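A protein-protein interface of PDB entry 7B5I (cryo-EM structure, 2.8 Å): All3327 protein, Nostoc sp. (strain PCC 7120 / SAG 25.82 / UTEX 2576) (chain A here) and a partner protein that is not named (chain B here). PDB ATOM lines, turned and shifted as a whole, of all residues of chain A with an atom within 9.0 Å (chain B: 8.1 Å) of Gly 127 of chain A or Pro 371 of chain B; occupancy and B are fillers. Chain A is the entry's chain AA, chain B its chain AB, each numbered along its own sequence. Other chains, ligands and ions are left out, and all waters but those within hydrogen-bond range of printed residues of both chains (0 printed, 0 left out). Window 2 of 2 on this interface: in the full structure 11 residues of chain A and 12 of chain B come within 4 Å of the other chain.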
ATOM      1  N   ARG A   7       8.716  -2.245  21.597  1.00  0.00           N
ATOM      2  CA  ARG A   7       7.738  -3.265  21.965  1.00  0.00           C
ATOM      3  C   ARG A   7       7.650  -4.357  20.907  1.00  0.00           C
ATOM      4  O   ARG A   7       7.543  -5.544  21.242  1.00  0.00           O
ATOM      5  CB  ARG A   7       6.372  -2.633  22.196  1.00  0.00           C
ATOM      6  CG  ARG A   7       6.149  -2.189  23.617  1.00  0.00           C
ATOM      7  CD  ARG A   7       4.678  -2.001  23.882  1.00  0.00           C
ATOM      8  NE  ARG A   7       4.175  -0.788  23.245  1.00  0.00           N
ATOM      9  CZ  ARG A   7       4.073   0.386  23.858  1.00  0.00           C
ATOM     10  NH1 ARG A   7       4.437   0.508  25.127  1.00  0.00           N
ATOM     11  NH2 ARG A   7       3.609   1.438  23.202  1.00  0.00           N
ATOM     12  N   LEU A   8       7.698  -3.978  19.628  1.00  0.00           N
ATOM     13  CA  LEU A   8       7.697  -4.970  18.555  1.00  0.00           C
ATOM     14  C   LEU A   8       8.876  -5.929  18.692  1.00  0.00           C
ATOM     15  O   LEU A   8       8.707  -7.161  18.673  1.00  0.00           O
ATOM     16  CB  LEU A   8       7.730  -4.257  17.203  1.00  0.00           C
ATOM     17  CG  LEU A   8       7.865  -5.079  15.919  1.00  0.00           C
ATOM     18  CD1 LEU A   8       6.686  -6.013  15.741  1.00  0.00           C
ATOM     19  CD2 LEU A   8       8.000  -4.168  14.714  1.00  0.00           C
ATOM     20  N   GLN A  10      10.714  -6.551  21.300  1.00  0.00           N
ATOM     21  CA  GLN A  10      10.607  -7.328  22.527  1.00  0.00           C
ATOM     22  C   GLN A  10       9.680  -8.517  22.347  1.00  0.00           C
ATOM     23  O   GLN A  10      10.010  -9.640  22.738  1.00  0.00           O
ATOM     24  CB  GLN A  10      10.112  -6.441  23.664  1.00  0.00           C
ATOM     25  CG  GLN A  10       9.967  -7.179  24.968  1.00  0.00           C
ATOM     26  CD  GLN A  10       8.986  -6.521  25.897  1.00  0.00           C
ATOM     27  OE1 GLN A  10       8.159  -5.716  25.474  1.00  0.00           O
ATOM     28  NE2 GLN A  10       9.065  -6.858  27.175  1.00  0.00           N
ATOM     29  N   VAL A  11       8.506  -8.286  21.758  1.00  0.00           N
ATOM     30  CA  VAL A  11       7.539  -9.366  21.605  1.00  0.00           C
ATOM     31  C   VAL A  11       8.096 -10.466  20.710  1.00  0.00           C
ATOM     32  O   VAL A  11       7.994 -11.659  21.034  1.00  0.00           O
ATOM     33  CB  VAL A  11       6.209  -8.809  21.072  1.00  0.00           C
ATOM     34  CG1 VAL A  11       5.284  -9.933  20.671  1.00  0.00           C
ATOM     35  CG2 VAL A  11       5.551  -7.950  22.132  1.00  0.00           C
ATOM     36  N   ALA A  12       8.723 -10.090  19.592  1.00  0.00           N
ATOM     37  CA  ALA A  12       9.235 -11.109  18.676  1.00  0.00           C
ATOM     38  C   ALA A  12      10.340 -11.939  19.325  1.00  0.00           C
ATOM     39  O   ALA A  12      10.344 -13.178  19.236  1.00  0.00           O
ATOM     40  CB  ALA A  12       9.730 -10.456  17.390  1.00  0.00           C
ATOM     41  N   LEU A  13      11.293 -11.275  19.986  1.00  0.00           N
ATOM     42  CA  LEU A  13      12.398 -12.010  20.593  1.00  0.00           C
ATOM     43  C   LEU A  13      11.915 -12.885  21.741  1.00  0.00           C
ATOM     44  O   LEU A  13      12.400 -14.010  21.919  1.00  0.00           O
ATOM     45  CB  LEU A  13      13.469 -11.037  21.075  1.00  0.00           C
ATOM     46  CG  LEU A  13      14.675 -11.652  21.783  1.00  0.00           C
ATOM     47  CD1 LEU A  13      15.549 -12.426  20.811  1.00  0.00           C
ATOM     48  CD2 LEU A  13      15.471 -10.581  22.496  1.00  0.00           C
ATOM     49  N   ARG A  15       8.995 -14.320  21.965  1.00  0.00           N
ATOM     50  CA  ARG A  15       8.365 -15.487  21.364  1.00  0.00           C
ATOM     51  C   ARG A  15       9.405 -16.510  20.926  1.00  0.00           C
ATOM     52  O   ARG A  15       9.294 -17.699  21.243  1.00  0.00           O
ATOM     53  CB  ARG A  15       7.503 -15.045  20.185  1.00  0.00           C
ATOM     54  CG  ARG A  15       6.705 -16.142  19.536  1.00  0.00           C
ATOM     55  CD  ARG A  15       5.600 -15.539  18.701  1.00  0.00           C
ATOM     56  NE  ARG A  15       4.938 -16.529  17.864  1.00  0.00           N
ATOM     57  CZ  ARG A  15       3.842 -16.290  17.156  1.00  0.00           C
ATOM     58  NH1 ARG A  15       3.281 -15.091  17.190  1.00  0.00           N
ATOM     59  NH2 ARG A  15       3.308 -17.249  16.414  1.00  0.00           N
ATOM     60  N   SER A 121       8.467  -6.134  10.988  1.00  0.00           N
ATOM     61  CA  SER A 121       7.288  -5.377  10.602  1.00  0.00           C
ATOM     62  C   SER A 121       6.072  -6.086  11.166  1.00  0.00           C
ATOM     63  O   SER A 121       6.133  -7.260  11.536  1.00  0.00           O
ATOM     64  CB  SER A 121       7.181  -5.239   9.081  1.00  0.00           C
ATOM     65  OG  SER A 121       6.008  -4.541   8.719  1.00  0.00           O
ATOM     66  N   PHE A 122       4.964  -5.351  11.234  1.00  0.00           N
ATOM     67  CA  PHE A 122       3.724  -5.950  11.709  1.00  0.00           C
ATOM     68  C   PHE A 122       3.203  -7.007  10.742  1.00  0.00           C
ATOM     69  O   PHE A 122       2.469  -7.911  11.151  1.00  0.00           O
ATOM     70  CB  PHE A 122       2.673  -4.866  11.935  1.00  0.00           C
ATOM     71  CG  PHE A 122       1.354  -5.397  12.402  1.00  0.00           C
ATOM     72  CD1 PHE A 122       1.175  -5.757  13.724  1.00  0.00           C
ATOM     73  CD2 PHE A 122       0.293  -5.533  11.524  1.00  0.00           C
ATOM     74  CE1 PHE A 122      -0.033  -6.248  14.162  1.00  0.00           C
ATOM     75  CE2 PHE A 122      -0.920  -6.022  11.957  1.00  0.00           C
ATOM     76  CZ  PHE A 122      -1.084  -6.381  13.278  1.00  0.00           C
ATOM     77  N   THR A 123       3.564  -6.916   9.467  1.00  0.00           N
ATOM     78  CA  THR A 123       3.079  -7.848   8.460  1.00  0.00           C
ATOM     79  C   THR A 123       3.863  -9.156   8.451  1.00  0.00           C
ATOM     80  O   THR A 123       3.371 -10.156   7.919  1.00  0.00           O
ATOM     81  CB  THR A 123       3.142  -7.186   7.078  1.00  0.00           C
ATOM     82  OG1 THR A 123       2.447  -5.937   7.123  1.00  0.00           O
ATOM     83  CG2 THR A 123       2.499  -8.048   6.011  1.00  0.00           C
ATOM     84  N   THR A 124       5.036  -9.189   9.072  1.00  0.00           N
ATOM     85  CA  THR A 124       5.902 -10.356   9.049  1.00  0.00           C
ATOM     86  C   THR A 124       6.243 -10.891  10.431  1.00  0.00           C
ATOM     87  O   THR A 124       6.535 -12.078  10.560  1.00  0.00           O
ATOM     88  CB  THR A 124       7.212 -10.042   8.307  1.00  0.00           C
ATOM     89  OG1 THR A 124       8.115  -9.381   9.195  1.00  0.00           O
ATOM     90  CG2 THR A 124       6.949  -9.137   7.116  1.00  0.00           C
ATOM     91  N   THR A 125       6.220 -10.052  11.460  1.00  0.00           N
ATOM     92  CA  THR A 125       6.477 -10.466  12.838  1.00  0.00           C
ATOM     93  C   THR A 125       5.345  -9.951  13.712  1.00  0.00           C
ATOM     94  O   THR A 125       5.542  -9.053  14.539  1.00  0.00           O
ATOM     95  CB  THR A 125       7.824  -9.942  13.337  1.00  0.00           C
ATOM     96  OG1 THR A 125       7.898  -8.529  13.115  1.00  0.00           O
ATOM     97  CG2 THR A 125       8.971 -10.621  12.619  1.00  0.00           C
ATOM     98  N   PRO A 126       4.138 -10.506  13.553  1.00  0.00           N
ATOM     99  CA  PRO A 126       2.952  -9.901  14.177  1.00  0.00           C
ATOM    100  C   PRO A 126       2.938  -9.965  15.697  1.00  0.00           C
ATOM    101  O   PRO A 126       2.782  -8.935  16.362  1.00  0.00           O
ATOM    102  CB  PRO A 126       1.795 -10.711  13.579  1.00  0.00           C
ATOM    103  CG  PRO A 126       2.394 -12.010  13.205  1.00  0.00           C
ATOM    104  CD  PRO A 126       3.811 -11.727  12.796  1.00  0.00           C
ATOM    105  N   GLY A 127       3.107 -11.155  16.260  1.00  0.00           N
ATOM    106  CA  GLY A 127       3.056 -11.326  17.700  1.00  0.00           C
ATOM    107  C   GLY A 127       1.711 -10.972  18.302  1.00  0.00           C
ATOM    108  O   GLY A 127       1.592 -10.783  19.512  1.00  0.00           O
ATOM    109  N   TYR B 323       1.008 -23.350   5.319  1.00  0.00           N
ATOM    110  CA  TYR B 323       2.016 -23.207   6.357  1.00  0.00           C
ATOM    111  C   TYR B 323       2.801 -24.505   6.473  1.00  0.00           C
ATOM    112  O   TYR B 323       2.214 -25.579   6.681  1.00  0.00           O
ATOM    113  CB  TYR B 323       1.361 -22.841   7.685  1.00  0.00           C
ATOM    114  CG  TYR B 323       0.820 -21.439   7.680  1.00  0.00           C
ATOM    115  CD1 TYR B 323       1.650 -20.356   7.916  1.00  0.00           C
ATOM    116  CD2 TYR B 323      -0.514 -21.191   7.404  1.00  0.00           C
ATOM    117  CE1 TYR B 323       1.162 -19.070   7.901  1.00  0.00           C
ATOM    118  CE2 TYR B 323      -1.010 -19.908   7.383  1.00  0.00           C
ATOM    119  CZ  TYR B 323      -0.166 -18.850   7.630  1.00  0.00           C
ATOM    120  OH  TYR B 323      -0.654 -17.565   7.613  1.00  0.00           O
ATOM    121  N   LEU B 363      -5.150 -10.976  10.178  1.00  0.00           N
ATOM    122  CA  LEU B 363      -4.437 -12.209   9.982  1.00  0.00           C
ATOM    123  C   LEU B 363      -5.147 -13.340  10.725  1.00  0.00           C
ATOM    124  O   LEU B 363      -5.941 -13.101  11.614  1.00  0.00           O
ATOM    125  CB  LEU B 363      -3.018 -12.042  10.524  1.00  0.00           C
ATOM    126  CG  LEU B 363      -2.066 -11.044   9.856  1.00  0.00           C
ATOM    127  CD1 LEU B 363      -2.672  -9.663   9.732  1.00  0.00           C
ATOM    128  CD2 LEU B 363      -0.773 -10.933  10.636  1.00  0.00           C
ATOM    129  N   LEU B 364      -4.796 -14.558  10.352  1.00  0.00           N
ATOM    130  CA  LEU B 364      -5.315 -15.804  10.876  1.00  0.00           C
ATOM    131  C   LEU B 364      -4.735 -16.184  12.243  1.00  0.00           C
ATOM    132  O   LEU B 364      -3.603 -15.862  12.511  1.00  0.00           O
ATOM    133  CB  LEU B 364      -4.917 -16.867   9.879  1.00  0.00           C
ATOM    134  CG  LEU B 364      -5.696 -16.886   8.575  1.00  0.00           C
ATOM    135  CD1 LEU B 364      -6.671 -15.742   8.525  1.00  0.00           C
ATOM    136  CD2 LEU B 364      -4.796 -16.867   7.362  1.00  0.00           C
ATOM    137  N   ASN B 365      -5.503 -16.859  13.106  1.00  0.00           N
ATOM    138  CA  ASN B 365      -4.990 -17.259  14.411  1.00  0.00           C
ATOM    139  C   ASN B 365      -4.710 -18.756  14.481  1.00  0.00           C
ATOM    140  O   ASN B 365      -5.373 -19.553  13.819  1.00  0.00           O
ATOM    141  CB  ASN B 365      -5.964 -16.852  15.518  1.00  0.00           C
ATOM    142  CG  ASN B 365      -7.319 -17.516  15.376  1.00  0.00           C
ATOM    143  OD1 ASN B 365      -7.561 -18.262  14.427  1.00  0.00           O
ATOM    144  ND2 ASN B 365      -8.212 -17.248  16.322  1.00  0.00           N
ATOM    145  N   ASP B 366      -3.724 -19.129  15.289  1.00  0.00           N
ATOM    146  CA  ASP B 366      -3.354 -20.506  15.446  1.00  0.00           C
ATOM    147  C   ASP B 366      -4.183 -21.201  16.515  1.00  0.00           C
ATOM    148  O   ASP B 366      -4.792 -20.551  17.367  1.00  0.00           O
ATOM    149  CB  ASP B 366      -1.891 -20.542  15.843  1.00  0.00           C
ATOM    150  CG  ASP B 366      -1.210 -21.766  15.366  1.00  0.00           C
ATOM    151  OD1 ASP B 366      -0.056 -22.013  15.777  1.00  0.00           O
ATOM    152  OD2 ASP B 366      -1.858 -22.496  14.591  1.00  0.00           O
ATOM    153  N   GLN B 368      -3.366 -22.368  19.130  1.00  0.00           N
ATOM    154  CA  GLN B 368      -2.887 -21.910  20.432  1.00  0.00           C
ATOM    155  C   GLN B 368      -3.074 -20.386  20.557  1.00  0.00           C
ATOM    156  O   GLN B 368      -2.532 -19.756  21.467  1.00  0.00           O
ATOM    157  CB  GLN B 368      -1.424 -22.300  20.647  1.00  0.00           C
ATOM    158  CG  GLN B 368      -0.940 -22.100  22.073  1.00  0.00           C
ATOM    159  CD  GLN B 368       0.338 -22.861  22.367  1.00  0.00           C
ATOM    160  OE1 GLN B 368       0.878 -22.787  23.471  1.00  0.00           O
ATOM    161  NE2 GLN B 368       0.828 -23.598  21.378  1.00  0.00           N
ATOM    162  N   ASP B 369      -3.885 -19.844  19.647  1.00  0.00           N
ATOM    163  CA  ASP B 369      -4.218 -18.418  19.569  1.00  0.00           C
ATOM    164  C   ASP B 369      -3.003 -17.506  19.415  1.00  0.00           C
ATOM    165  O   ASP B 369      -2.607 -16.810  20.350  1.00  0.00           O
ATOM    166  CB  ASP B 369      -5.103 -17.973  20.744  1.00  0.00           C
ATOM    167  CG  ASP B 369      -6.417 -18.727  20.802  1.00  0.00           C
ATOM    168  OD1 ASP B 369      -6.650 -19.584  19.924  1.00  0.00           O
ATOM    169  OD2 ASP B 369      -7.216 -18.462  21.724  1.00  0.00           O
ATOM    170  N   ARG B 370      -2.422 -17.518  18.218  1.00  0.00           N
ATOM    171  CA  ARG B 370      -1.262 -16.693  17.897  1.00  0.00           C
ATOM    172  C   ARG B 370      -1.337 -16.237  16.443  1.00  0.00           C
ATOM    173  O   ARG B 370      -1.650 -17.030  15.556  1.00  0.00           O
ATOM    174  CB  ARG B 370       0.042 -17.461  18.126  1.00  0.00           C
ATOM    175  CG  ARG B 370       0.384 -17.722  19.583  1.00  0.00           C
ATOM    176  CD  ARG B 370       1.842 -18.127  19.735  1.00  0.00           C
ATOM    177  NE  ARG B 370       2.139 -18.623  21.075  1.00  0.00           N
ATOM    178  CZ  ARG B 370       2.216 -19.911  21.394  1.00  0.00           C
ATOM    179  NH1 ARG B 370       2.023 -20.837  20.464  1.00  0.00           N
ATOM    180  NH2 ARG B 370       2.490 -20.273  22.639  1.00  0.00           N
ATOM    181  N   PRO B 371      -1.049 -14.951  16.195  1.00  0.00           N
ATOM    182  CA  PRO B 371      -1.081 -14.405  14.834  1.00  0.00           C
ATOM    183  C   PRO B 371       0.010 -15.030  13.971  1.00  0.00           C
ATOM    184  O   PRO B 371       1.129 -15.217  14.450  1.00  0.00           O
ATOM    185  CB  PRO B 371      -0.800 -12.915  15.047  1.00  0.00           C
ATOM    186  CG  PRO B 371      -0.066 -12.847  16.344  1.00  0.00           C
ATOM    187  CD  PRO B 371      -0.646 -13.942  17.190  1.00  0.00           C
ATOM    188  N   LEU B 372      -0.309 -15.348  12.721  1.00  0.00           N
ATOM    189  CA  LEU B 372       0.662 -15.952  11.838  1.00  0.00           C
ATOM    190  C   LEU B 372       1.052 -14.977  10.737  1.00  0.00           C
ATOM    191  O   LEU B 372       0.199 -14.238  10.240  1.00  0.00           O
ATOM    192  CB  LEU B 372       0.093 -17.227  11.213  1.00  0.00           C
ATOM    193  CG  LEU B 372      -0.195 -18.350  12.198  1.00  0.00           C
ATOM    194  CD1 LEU B 372      -0.974 -19.452  11.521  1.00  0.00           C
ATOM    195  CD2 LEU B 372       1.111 -18.884  12.748  1.00  0.00           C
ATOM    196  N   PRO B 373       2.322 -14.947  10.340  1.00  0.00           N
ATOM    197  CA  PRO B 373       2.734 -14.035   9.268  1.00  0.00           C
ATOM    198  C   PRO B 373       2.025 -14.339   7.958  1.00  0.00           C
ATOM    199  O   PRO B 373       1.674 -15.483   7.664  1.00  0.00           O
ATOM    200  CB  PRO B 373       4.243 -14.281   9.154  1.00  0.00           C
ATOM    201  CG  PRO B 373       4.488 -15.573   9.846  1.00  0.00           C
ATOM    202  CD  PRO B 373       3.464 -15.666  10.919  1.00  0.00           C
ATOM    203  N   ALA B 374       1.824 -13.294   7.168  1.00  0.00           N
ATOM    204  CA  ALA B 374       1.214 -13.412   5.855  1.00  0.00           C
ATOM    205  C   ALA B 374       2.250 -13.891   4.849  1.00  0.00           C
ATOM    206  O   ALA B 374       3.451 -13.856   5.113  1.00  0.00           O
ATOM    207  CB  ALA B 374       0.624 -12.065   5.446  1.00  0.00           C
ATOM    208  N   LEU B 399       7.796 -21.575   8.495  1.00  0.00           N
ATOM    209  CA  LEU B 399       7.859 -21.097   9.866  1.00  0.00           C
ATOM    210  C   LEU B 399       9.040 -21.713  10.597  1.00  0.00           C
ATOM    211  O   LEU B 399       9.642 -22.673  10.118  1.00  0.00           O
ATOM    212  CB  LEU B 399       6.561 -21.420  10.599  1.00  0.00           C
ATOM    213  CG  LEU B 399       5.294 -20.766  10.052  1.00  0.00           C
ATOM    214  CD1 LEU B 399       4.070 -21.485  10.577  1.00  0.00           C
ATOM    215  CD2 LEU B 399       5.250 -19.302  10.427  1.00  0.00           C
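Among the printed residues, merely in contact across the chains: Arg 15 of chain A with Arg 370 of chain B (3.7 Å), Thr 123 of chain A with Ala 374 of chain B (3.6 Å), Thr 124 of chain A with Pro 373 of chain B (3.5 Å), Pro 126 of chain A with Leu 363 of chain B (3.9 Å), Pro 126 of chain A with Pro 371 of chain B (3.7 Å) and Gly 127 of chain A with Pro 371 of chain B (3.2 Å).
The backbone NH (N) of Thr 123 of chain A sits close to the side-chain hydroxyl (OG) of Ser 121 of chain A (3.5 Å). OE1 of Gln 368 of chain B is in hydrogen-bond range of NH2 of Arg 370 of chain B (3.1 Å). OH of Tyr 323 of chain B is in hydrogen-bond range of O of Pro 373 of chain B (3.1 Å).
Printed residues of chain A that touch a printed residue of chain B: Arg 15, Thr 123, Thr 124, Pro 126 and Gly 127. Among the printed residues, no Asp or Glu carboxylate lies within 4 Å of a Lys or Arg side-chain nitrogen of the other chain.
The backbone carbonyl oxygen (O) of Pro 371 of chain B lies within hydrogen-bond range of the guanidinium group (NH1) of Arg 15 of chain A, at 3.5 Å.
Ala 12 of chain A touches none of the printed residues of chain B. Of the printed residues of chain B, Arg 15 of chain A touches Arg 370 and Pro 371. Of the printed residues of chain B, Thr 124 of chain A touches Pro 373. Of chain B, only Leu 363 (3.9 Å) and Pro 371 (3.7 Å) come within 4 Å of Pro 126 of chain A. Of chain B, only Pro 371 (3.2 Å) comes within 4 Å of Gly 127 of chain A. Printed residues of chain A within 4 Å of Leu 363 of chain B: Pro 126 (3.9 Å). Leu 364 of chain B touches none of the printed residues of chain A. Of chain A, only Arg 15, Pro 126 and Gly 127 come within 4 Å of Pro 371 of chain B. Of the printed residues of chain A, Pro 373 of chain B touches Thr 124. The nearest residue of chain A that does not touch Pro 371 of chain B is Thr 125 of chain A (6.7 Å).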
